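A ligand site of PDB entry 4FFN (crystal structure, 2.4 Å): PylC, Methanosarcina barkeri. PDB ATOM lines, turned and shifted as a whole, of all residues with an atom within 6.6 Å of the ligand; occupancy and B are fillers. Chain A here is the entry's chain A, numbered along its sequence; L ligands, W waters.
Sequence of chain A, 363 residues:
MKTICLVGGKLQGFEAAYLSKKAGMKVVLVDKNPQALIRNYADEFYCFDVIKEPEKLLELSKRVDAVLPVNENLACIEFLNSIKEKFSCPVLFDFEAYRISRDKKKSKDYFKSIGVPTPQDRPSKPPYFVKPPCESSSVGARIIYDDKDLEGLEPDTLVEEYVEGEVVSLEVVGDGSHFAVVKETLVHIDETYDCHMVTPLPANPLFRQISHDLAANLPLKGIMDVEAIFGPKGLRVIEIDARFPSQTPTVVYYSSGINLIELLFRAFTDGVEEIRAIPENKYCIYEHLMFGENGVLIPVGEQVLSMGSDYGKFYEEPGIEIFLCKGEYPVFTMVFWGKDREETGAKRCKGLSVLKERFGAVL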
ATOM      1  N   VAL A   7     -31.913  -0.082   1.021  1.00  0.00           N
ATOM      2  CA  VAL A   7     -31.658  -0.291   2.441  1.00  0.00           C
ATOM      3  C   VAL A   7     -30.691  -1.445   2.615  1.00  0.00           C
ATOM      4  O   VAL A   7     -31.064  -2.620   2.601  1.00  0.00           O
ATOM      5  CB  VAL A   7     -32.950  -0.483   3.242  1.00  0.00           C
ATOM      6  CG1 VAL A   7     -32.638  -0.714   4.717  1.00  0.00           C
ATOM      7  CG2 VAL A   7     -33.845   0.732   3.070  1.00  0.00           C
ATOM      8  N   GLY A   8     -29.421  -1.077   2.781  1.00  0.00           N
ATOM      9  CA  GLY A   8     -28.323  -2.033   2.781  1.00  0.00           C
ATOM     10  C   GLY A   8     -27.214  -1.678   1.805  1.00  0.00           C
ATOM     11  O   GLY A   8     -27.432  -1.593   0.580  1.00  0.00           O
ATOM     12  N   GLY A   9     -26.020  -1.506   2.360  1.00  0.00           N
ATOM     13  CA  GLY A   9     -24.859  -1.051   1.616  1.00  0.00           C
ATOM     14  C   GLY A   9     -23.724  -2.032   1.431  1.00  0.00           C
ATOM     15  O   GLY A   9     -22.567  -1.637   1.299  1.00  0.00           O
ATOM     16  N   LYS A  10     -24.013  -3.319   1.392  1.00  0.00           N
ATOM     17  CA  LYS A  10     -22.932  -4.249   1.156  1.00  0.00           C
ATOM     18  C   LYS A  10     -22.975  -4.822  -0.252  1.00  0.00           C
ATOM     19  O   LYS A  10     -23.001  -4.050  -1.214  1.00  0.00           O
ATOM     20  CB  LYS A  10     -22.834  -5.291   2.262  1.00  0.00           C
ATOM     21  CG  LYS A  10     -22.360  -4.629   3.552  1.00  0.00           C
ATOM     22  CD  LYS A  10     -22.279  -5.580   4.727  1.00  0.00           C
ATOM     23  CE  LYS A  10     -21.059  -6.469   4.650  1.00  0.00           C
ATOM     24  NZ  LYS A  10     -20.487  -6.690   6.004  1.00  0.00           N
ATOM     25  N   LEU A  11     -22.985  -6.156  -0.357  1.00  0.00           N
ATOM     26  CA  LEU A  11     -22.888  -6.846  -1.660  1.00  0.00           C
ATOM     27  C   LEU A  11     -24.207  -6.893  -2.409  1.00  0.00           C
ATOM     28  O   LEU A  11     -24.248  -6.623  -3.614  1.00  0.00           O
ATOM     29  CB  LEU A  11     -22.325  -8.265  -1.475  1.00  0.00           C
ATOM     30  CG  LEU A  11     -20.934  -8.377  -0.857  1.00  0.00           C
ATOM     31  CD1 LEU A  11     -20.558  -9.820  -0.546  1.00  0.00           C
ATOM     32  CD2 LEU A  11     -19.879  -7.720  -1.744  1.00  0.00           C
ATOM     33  N   GLN A  12     -25.280  -7.232  -1.709  1.00  0.00           N
ATOM     34  CA  GLN A  12     -26.605  -7.082  -2.284  1.00  0.00           C
ATOM     35  C   GLN A  12     -26.734  -5.655  -2.779  1.00  0.00           C
ATOM     36  O   GLN A  12     -27.076  -5.428  -3.936  1.00  0.00           O
ATOM     37  CB  GLN A  12     -27.689  -7.353  -1.260  1.00  0.00           C
ATOM     38  CG  GLN A  12     -28.076  -8.798  -1.055  1.00  0.00           C
ATOM     39  CD  GLN A  12     -29.212  -8.884  -0.073  1.00  0.00           C
ATOM     40  OE1 GLN A  12     -28.989  -8.864   1.130  1.00  0.00           O
ATOM     41  NE2 GLN A  12     -30.446  -8.921  -0.583  1.00  0.00           N
ATOM     42  N   VAL A  30     -29.311   3.948   2.214  1.00  0.00           N
ATOM     43  CA  VAL A  30     -29.499   4.079   3.640  1.00  0.00           C
ATOM     44  C   VAL A  30     -28.768   2.895   4.243  1.00  0.00           C
ATOM     45  O   VAL A  30     -28.951   1.768   3.800  1.00  0.00           O
ATOM     46  CB  VAL A  30     -30.975   3.940   4.031  1.00  0.00           C
ATOM     47  CG1 VAL A  30     -31.112   4.008   5.539  1.00  0.00           C
ATOM     48  CG2 VAL A  30     -31.824   5.011   3.362  1.00  0.00           C
ATOM     49  N   ASP A  31     -27.955   3.170   5.258  1.00  0.00           N
ATOM     50  CA  ASP A  31     -27.233   2.119   5.979  1.00  0.00           C
ATOM     51  C   ASP A  31     -26.847   2.677   7.342  1.00  0.00           C
ATOM     52  O   ASP A  31     -26.492   3.850   7.453  1.00  0.00           O
ATOM     53  CB  ASP A  31     -25.995   1.681   5.187  1.00  0.00           C
ATOM     54  CG  ASP A  31     -25.478   0.297   5.596  1.00  0.00           C
ATOM     55  OD1 ASP A  31     -25.044   0.128   6.763  1.00  0.00           O
ATOM     56  OD2 ASP A  31     -25.481  -0.616   4.743  1.00  0.00           O
ATOM     57  N   LYS A  32     -26.933   1.839   8.369  1.00  0.00           N
ATOM     58  CA  LYS A  32     -26.649   2.256   9.751  1.00  0.00           C
ATOM     59  C   LYS A  32     -25.141   2.340  10.005  1.00  0.00           C
ATOM     60  O   LYS A  32     -24.691   2.831  11.033  1.00  0.00           O
ATOM     61  CB  LYS A  32     -27.308   1.282  10.753  1.00  0.00           C
ATOM     62  CG  LYS A  32     -26.819  -0.152  10.567  1.00  0.00           C
ATOM     63  CD  LYS A  32     -27.364  -1.205  11.516  1.00  0.00           C
ATOM     64  CE  LYS A  32     -26.930  -2.570  10.994  1.00  0.00           C
ATOM     65  NZ  LYS A  32     -27.773  -3.706  11.459  1.00  0.00           N
ATOM     66  N   ASN A  33     -24.352   1.829   9.066  1.00  0.00           N
ATOM     67  CA  ASN A  33     -22.900   1.812   9.223  1.00  0.00           C
ATOM     68  C   ASN A  33     -22.270   3.003   8.463  1.00  0.00           C
ATOM     69  O   ASN A  33     -22.443   3.123   7.251  1.00  0.00           O
ATOM     70  CB  ASN A  33     -22.353   0.444   8.796  1.00  0.00           C
ATOM     71  CG  ASN A  33     -20.839   0.331   8.875  1.00  0.00           C
ATOM     72  OD1 ASN A  33     -20.120   1.287   9.196  1.00  0.00           O
ATOM     73  ND2 ASN A  33     -20.329  -0.850   8.558  1.00  0.00           N
ATOM     74  N   ALA A  36     -20.354   1.967   5.716  1.00  0.00           N
ATOM     75  CA  ALA A  36     -21.009   1.136   4.691  1.00  0.00           C
ATOM     76  C   ALA A  36     -20.148   0.943   3.429  1.00  0.00           C
ATOM     77  O   ALA A  36     -19.662   1.912   2.856  1.00  0.00           O
ATOM     78  CB  ALA A  36     -22.372   1.705   4.315  1.00  0.00           C
ATOM     79  N   LEU A  37     -19.960  -0.313   3.026  1.00  0.00           N
ATOM     80  CA  LEU A  37     -19.081  -0.690   1.907  1.00  0.00           C
ATOM     81  C   LEU A  37     -19.187   0.154   0.625  1.00  0.00           C
ATOM     82  O   LEU A  37     -18.165   0.515   0.033  1.00  0.00           O
ATOM     83  CB  LEU A  37     -19.275  -2.168   1.566  1.00  0.00           C
ATOM     84  CG  LEU A  37     -18.212  -2.866   0.718  1.00  0.00           C
ATOM     85  CD1 LEU A  37     -16.859  -2.820   1.403  1.00  0.00           C
ATOM     86  CD2 LEU A  37     -18.595  -4.304   0.434  1.00  0.00           C
ATOM     87  N   PHE A  48     -28.249   5.979   8.769  1.00  0.00           N
ATOM     88  CA  PHE A  48     -29.125   5.804   9.932  1.00  0.00           C
ATOM     89  C   PHE A  48     -29.694   4.400   9.997  1.00  0.00           C
ATOM     90  O   PHE A  48     -29.856   3.736   8.980  1.00  0.00           O
ATOM     91  CB  PHE A  48     -30.251   6.856   9.984  1.00  0.00           C
ATOM     92  CG  PHE A  48     -31.245   6.762   8.845  1.00  0.00           C
ATOM     93  CD1 PHE A  48     -31.017   7.427   7.641  1.00  0.00           C
ATOM     94  CD2 PHE A  48     -32.438   6.054   8.995  1.00  0.00           C
ATOM     95  CE1 PHE A  48     -31.947   7.370   6.606  1.00  0.00           C
ATOM     96  CE2 PHE A  48     -33.367   5.980   7.960  1.00  0.00           C
ATOM     97  CZ  PHE A  48     -33.118   6.642   6.764  1.00  0.00           C
ATOM     98  N   ASP A  49     -30.010   3.963  11.208  1.00  0.00           N
ATOM     99  CA  ASP A  49     -30.684   2.692  11.364  1.00  0.00           C
ATOM    100  C   ASP A  49     -32.187   2.882  11.173  1.00  0.00           C
ATOM    101  O   ASP A  49     -32.801   3.718  11.849  1.00  0.00           O
ATOM    102  CB  ASP A  49     -30.395   2.097  12.736  1.00  0.00           C
ATOM    103  CG  ASP A  49     -30.844   0.662  12.843  1.00  0.00           C
ATOM    104  OD1 ASP A  49     -31.974   0.370  12.413  1.00  0.00           O
ATOM    105  OD2 ASP A  49     -30.065  -0.155  13.368  1.00  0.00           O
ATOM    106  N   VAL A  50     -32.790   2.104  10.263  1.00  0.00           N
ATOM    107  CA  VAL A  50     -34.195   2.336   9.870  1.00  0.00           C
ATOM    108  C   VAL A  50     -35.200   1.930  10.946  1.00  0.00           C
ATOM    109  O   VAL A  50     -36.292   2.480  10.992  1.00  0.00           O
ATOM    110  CB  VAL A  50     -34.610   1.716   8.504  1.00  0.00           C
ATOM    111  CG1 VAL A  50     -33.672   2.144   7.383  1.00  0.00           C
ATOM    112  CG2 VAL A  50     -34.737   0.187   8.577  1.00  0.00           C
ATOM    113  N   ILE A  51     -34.819   0.958  11.769  1.00  0.00           N
ATOM    114  CA  ILE A  51     -35.584   0.558  12.956  1.00  0.00           C
ATOM    115  C   ILE A  51     -35.592   1.667  14.007  1.00  0.00           C
ATOM    116  O   ILE A  51     -36.622   1.909  14.630  1.00  0.00           O
ATOM    117  CB  ILE A  51     -34.993  -0.707  13.627  1.00  0.00           C
ATOM    118  CG1 ILE A  51     -34.827  -1.849  12.641  1.00  0.00           C
ATOM    119  CG2 ILE A  51     -35.883  -1.158  14.777  1.00  0.00           C
ATOM    120  CD1 ILE A  51     -34.201  -3.081  13.261  1.00  0.00           C
ATOM    121  N   LYS A  52     -34.449   2.315  14.207  1.00  0.00           N
ATOM    122  CA  LYS A  52     -34.352   3.438  15.153  1.00  0.00           C
ATOM    123  C   LYS A  52     -35.011   4.729  14.670  1.00  0.00           C
ATOM    124  O   LYS A  52     -35.574   5.478  15.481  1.00  0.00           O
ATOM    125  CB  LYS A  52     -32.897   3.759  15.490  1.00  0.00           C
ATOM    126  CG  LYS A  52     -32.120   2.604  16.098  1.00  0.00           C
ATOM    127  CD  LYS A  52     -30.654   2.979  16.226  1.00  0.00           C
ATOM    128  CE  LYS A  52     -29.916   2.069  17.190  1.00  0.00           C
ATOM    129  NZ  LYS A  52     -28.452   2.061  16.922  1.00  0.00           N
ATOM    130  N   VAL A  70     -31.999  -4.393   0.755  1.00  0.00           N
ATOM    131  CA  VAL A  70     -30.929  -5.300   0.326  1.00  0.00           C
ATOM    132  C   VAL A  70     -30.051  -5.611   1.538  1.00  0.00           C
ATOM    133  O   VAL A  70     -28.938  -5.117   1.650  1.00  0.00           O
ATOM    134  CB  VAL A  70     -30.080  -4.738  -0.837  1.00  0.00           C
ATOM    135  CG1 VAL A  70     -30.608  -5.233  -2.183  1.00  0.00           C
ATOM    136  CG2 VAL A  70     -30.030  -3.219  -0.799  1.00  0.00           C
ATOM    137  N   ASN A  71     -30.612  -6.351   2.480  1.00  0.00           N
ATOM    138  CA  ASN A  71     -29.871  -6.848   3.621  1.00  0.00           C
ATOM    139  C   ASN A  71     -30.622  -8.071   4.072  1.00  0.00           C
ATOM    140  O   ASN A  71     -31.722  -8.342   3.586  1.00  0.00           O
ATOM    141  CB  ASN A  71     -29.725  -5.796   4.740  1.00  0.00           C
ATOM    142  CG  ASN A  71     -31.053  -5.439   5.403  1.00  0.00           C
ATOM    143  OD1 ASN A  71     -31.534  -6.141   6.277  1.00  0.00           O
ATOM    144  ND2 ASN A  71     -31.627  -4.317   4.972  1.00  0.00           N
ATOM    145  N   GLU A  72     -30.020  -8.812   4.995  1.00  0.00           N
ATOM    146  CA  GLU A  72     -30.523 -10.109   5.415  1.00  0.00           C
ATOM    147  C   GLU A  72     -30.564 -10.076   6.936  1.00  0.00           C
ATOM    148  O   GLU A  72     -30.510 -11.112   7.614  1.00  0.00           O
ATOM    149  CB  GLU A  72     -29.635 -11.237   4.865  1.00  0.00           C
ATOM    150  CG  GLU A  72     -29.908 -11.542   3.384  1.00  0.00           C
ATOM    151  CD  GLU A  72     -28.981 -12.577   2.756  1.00  0.00           C
ATOM    152  OE1 GLU A  72     -27.742 -12.370   2.776  1.00  0.00           O
ATOM    153  OE2 GLU A  72     -29.482 -13.587   2.195  1.00  0.00           O
ATOM    154  N   ASN A  73     -30.644  -8.859   7.445  1.00  0.00           N
ATOM    155  CA  ASN A  73     -30.824  -8.651   8.858  1.00  0.00           C
ATOM    156  C   ASN A  73     -32.301  -8.789   9.173  1.00  0.00           C
ATOM    157  O   ASN A  73     -33.120  -7.931   8.833  1.00  0.00           O
ATOM    158  CB  ASN A  73     -30.298  -7.288   9.282  1.00  0.00           C
ATOM    159  CG  ASN A  73     -30.642  -6.961  10.717  1.00  0.00           C
ATOM    160  OD1 ASN A  73     -31.254  -7.760  11.425  1.00  0.00           O
ATOM    161  ND2 ASN A  73     -30.264  -5.768  11.156  1.00  0.00           N
ATOM    162  N   LEU A  74     -32.619  -9.895   9.835  1.00  0.00           N
ATOM    163  CA  LEU A  74     -34.009 -10.296  10.057  1.00  0.00           C
ATOM    164  C   LEU A  74     -34.758  -9.303  10.924  1.00  0.00           C
ATOM    165  O   LEU A  74     -35.930  -9.059  10.711  1.00  0.00           O
ATOM    166  CB  LEU A  74     -34.118 -11.718  10.621  1.00  0.00           C
ATOM    167  CG  LEU A  74     -35.562 -12.237  10.709  1.00  0.00           C
ATOM    168  CD1 LEU A  74     -36.176 -12.474   9.337  1.00  0.00           C
ATOM    169  CD2 LEU A  74     -35.719 -13.462  11.597  1.00  0.00           C
ATOM    170  N   ALA A  75     -34.096  -8.680  11.895  1.00  0.00           N
ATOM    171  CA  ALA A  75     -34.745  -7.581  12.579  1.00  0.00           C
ATOM    172  C   ALA A  75     -35.147  -6.478  11.586  1.00  0.00           C
ATOM    173  O   ALA A  75     -36.205  -5.866  11.722  1.00  0.00           O
ATOM    174  CB  ALA A  75     -33.851  -7.017  13.666  1.00  0.00           C
ATOM    175  N   CYS A  76     -34.299  -6.219  10.593  1.00  0.00           N
ATOM    176  CA  CYS A  76     -34.571  -5.100   9.711  1.00  0.00           C
ATOM    177  C   CYS A  76     -35.801  -5.462   8.892  1.00  0.00           C
ATOM    178  O   CYS A  76     -36.793  -4.731   8.865  1.00  0.00           O
ATOM    179  CB  CYS A  76     -33.343  -4.765   8.844  1.00  0.00           C
ATOM    180  SG  CYS A  76     -33.585  -3.391   7.708  1.00  0.00           S
ATOM    181  N   SER A 306     -16.707  -8.923   1.601  1.00  0.00           N
ATOM    182  CA  SER A 306     -17.626  -8.294   2.536  1.00  0.00           C
ATOM    183  C   SER A 306     -16.950  -7.833   3.846  1.00  0.00           C
ATOM    184  O   SER A 306     -17.543  -7.094   4.631  1.00  0.00           O
ATOM    185  CB  SER A 306     -18.834  -9.179   2.804  1.00  0.00           C
ATOM    186  OG  SER A 306     -18.700  -9.903   4.011  1.00  0.00           O
HETATM  187  P1  LIG L   1     -22.850  -6.461   9.047  1.00  0.00           P
HETATM  188  O1  LIG L   1     -21.612  -5.776   8.514  1.00  0.00           O
HETATM  189  O2  LIG L   1     -22.600  -7.827   9.670  1.00  0.00           O
HETATM  190  O3  LIG L   1     -23.710  -5.540   9.896  1.00  0.00           O
HETATM  191  P2  LIG L   1     -23.932  -8.357   7.296  1.00  0.00           P
HETATM  192  O4  LIG L   1     -22.645  -8.817   6.644  1.00  0.00           O
HETATM  193  O5  LIG L   1     -24.481  -9.137   8.467  1.00  0.00           O
HETATM  194  O6  LIG L   1     -23.744  -6.815   7.741  1.00  0.00           O
HETATM  195  P3  LIG L   1     -26.554  -7.764   6.461  1.00  0.00           P
HETATM  196  O7  LIG L   1     -27.379  -8.378   5.352  1.00  0.00           O
HETATM  197  O8  LIG L   1     -26.912  -8.032   7.904  1.00  0.00           O
HETATM  198  O9  LIG L   1     -25.053  -8.245   6.155  1.00  0.00           O
HETATM  199  O10 LIG L   1     -26.558  -6.176   6.237  1.00  0.00           O
HETATM  200  C1  LIG L   1     -26.097  -5.645   5.002  1.00  0.00           C
HETATM  201  C2  LIG L   1     -26.056  -4.127   5.088  1.00  0.00           C
HETATM  202  O11 LIG L   1     -27.331  -3.595   5.469  1.00  0.00           O
HETATM  203  C3  LIG L   1     -25.053  -3.689   6.141  1.00  0.00           C
HETATM  204  O12 LIG L   1     -24.291  -2.616   5.610  1.00  0.00           O
HETATM  205  C4  LIG L   1     -25.926  -3.218   7.284  1.00  0.00           C
HETATM  206  O13 LIG L   1     -25.332  -2.162   8.012  1.00  0.00           O
HETATM  207  C5  LIG L   1     -27.167  -2.721   6.567  1.00  0.00           C
HETATM  208  N1  LIG L   1     -28.261  -2.789   7.548  1.00  0.00           N
HETATM  209  C6  LIG L   1     -28.639  -3.890   8.216  1.00  0.00           C
HETATM  210  N2  LIG L   1     -29.679  -3.609   9.058  1.00  0.00           N
HETATM  211  C7  LIG L   1     -29.963  -2.306   8.929  1.00  0.00           C
HETATM  212  C8  LIG L   1     -30.927  -1.345   9.536  1.00  0.00           C
HETATM  213  N3  LIG L   1     -31.823  -1.761  10.462  1.00  0.00           N
HETATM  214  N4  LIG L   1     -30.887  -0.059   9.122  1.00  0.00           N
HETATM  215  C9  LIG L   1     -29.994   0.374   8.196  1.00  0.00           C
HETATM  216  N5  LIG L   1     -29.087  -0.443   7.612  1.00  0.00           N
HETATM  217  C10 LIG L   1     -29.020  -1.756   7.936  1.00  0.00           C
HETATM  218  O   HOH W   1     -26.630  -6.132  10.057  1.00  0.00           O
HETATM  219  O   HOH W   2     -30.077  -2.954  12.666  1.00  0.00           O
HETATM  220  O   HOH W   3     -25.375  -9.078  10.896  1.00  0.00           O
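The side-chain carboxylate of Asp 31 lies within hydrogen-bond range of an oxygen (O12) of the ligand (2.5 Å).
N4 of the ligand lies within hydrogen-bond range of N of Val 50 (3.1 Å).
The backbone NH (N) of Lys 32 is in hydrogen-bond range of a nitrogen (N5) of the ligand (3.2 Å).
A nitrogen (N2) of the ligand is in hydrogen-bond range of the side-chain amide nitrogen of Asn 73.
The side-chain amino group of Lys 32 is in hydrogen-bond range of a nitrogen (N2) of the ligand, 3.1 Å away.
The backbone NH of Glu 72 lies within hydrogen-bond range of an oxygen (O7) of the ligand, 2.7 Å away.
NZ of Lys 10 is in salt-bridge range of O1 of the ligand, at 2.9 Å.
The side-chain sulfur (SG) of Cys 76 sits at hydrogen-bond distance from a nitrogen (N3) of the ligand, 3.7 Å away.
N3 of the ligand is in hydrogen-bond range of OD1 of Asp 49, at 2.9 Å.
N of Gly 8 lies within hydrogen-bond range of O of Val 30 (3.1 Å).
N of Asn 73 is in hydrogen-bond range of OD1 of Asn 71 (3.1 Å).
The side-chain carboxylate of Asp 31 is in hydrogen-bond range of the backbone NH of Asn 33.
The side-chain amide nitrogen (ND2) of Asn 71 is in hydrogen-bond range of the backbone carbonyl oxygen (O) of Val 7.
NZ of Lys 32 sits close to ND2 of Asn 73 (3.2 Å).
The backbone carbonyl oxygen (O) of Asp 31 lies within hydrogen-bond range of the backbone NH (N) of Phe 48 (3.1 Å).
The backbone NH (N) of Asn 71 sits at hydrogen-bond distance from the side-chain amide oxygen (OE1) of Gln 12, 3.3 Å away.
The side-chain amide oxygen (OD1) of Asn 73 sits at hydrogen-bond distance from the backbone NH (N) of Ala 75 (3.0 Å).
Gly 8 touches the ligand (CA to O11, 3.3 Å).
Gly 9 touches the ligand.
Phe 48 touches the ligand.
CG1 of Ile 51 touches N3 of the ligand, at 3.7 Å.
Asn 71 touches the ligand.
Hydrophobic or aromatic side chains that line the ligand: Val 50 and Ile 51.
13 residues have an atom within 4 Å of the ligand: Gly 8, Gly 9, Lys 10, Asp 31, Lys 32, Phe 48, Asp 49, Val 50, Ile 51, Asn 71, Glu 72, Asn 73 and Cys 76.
Water W1 lies within hydrogen-bond range of an oxygen (O8) of the ligand (2.9 Å) and the side-chain amino group of Lys 32 (3.0 Å).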
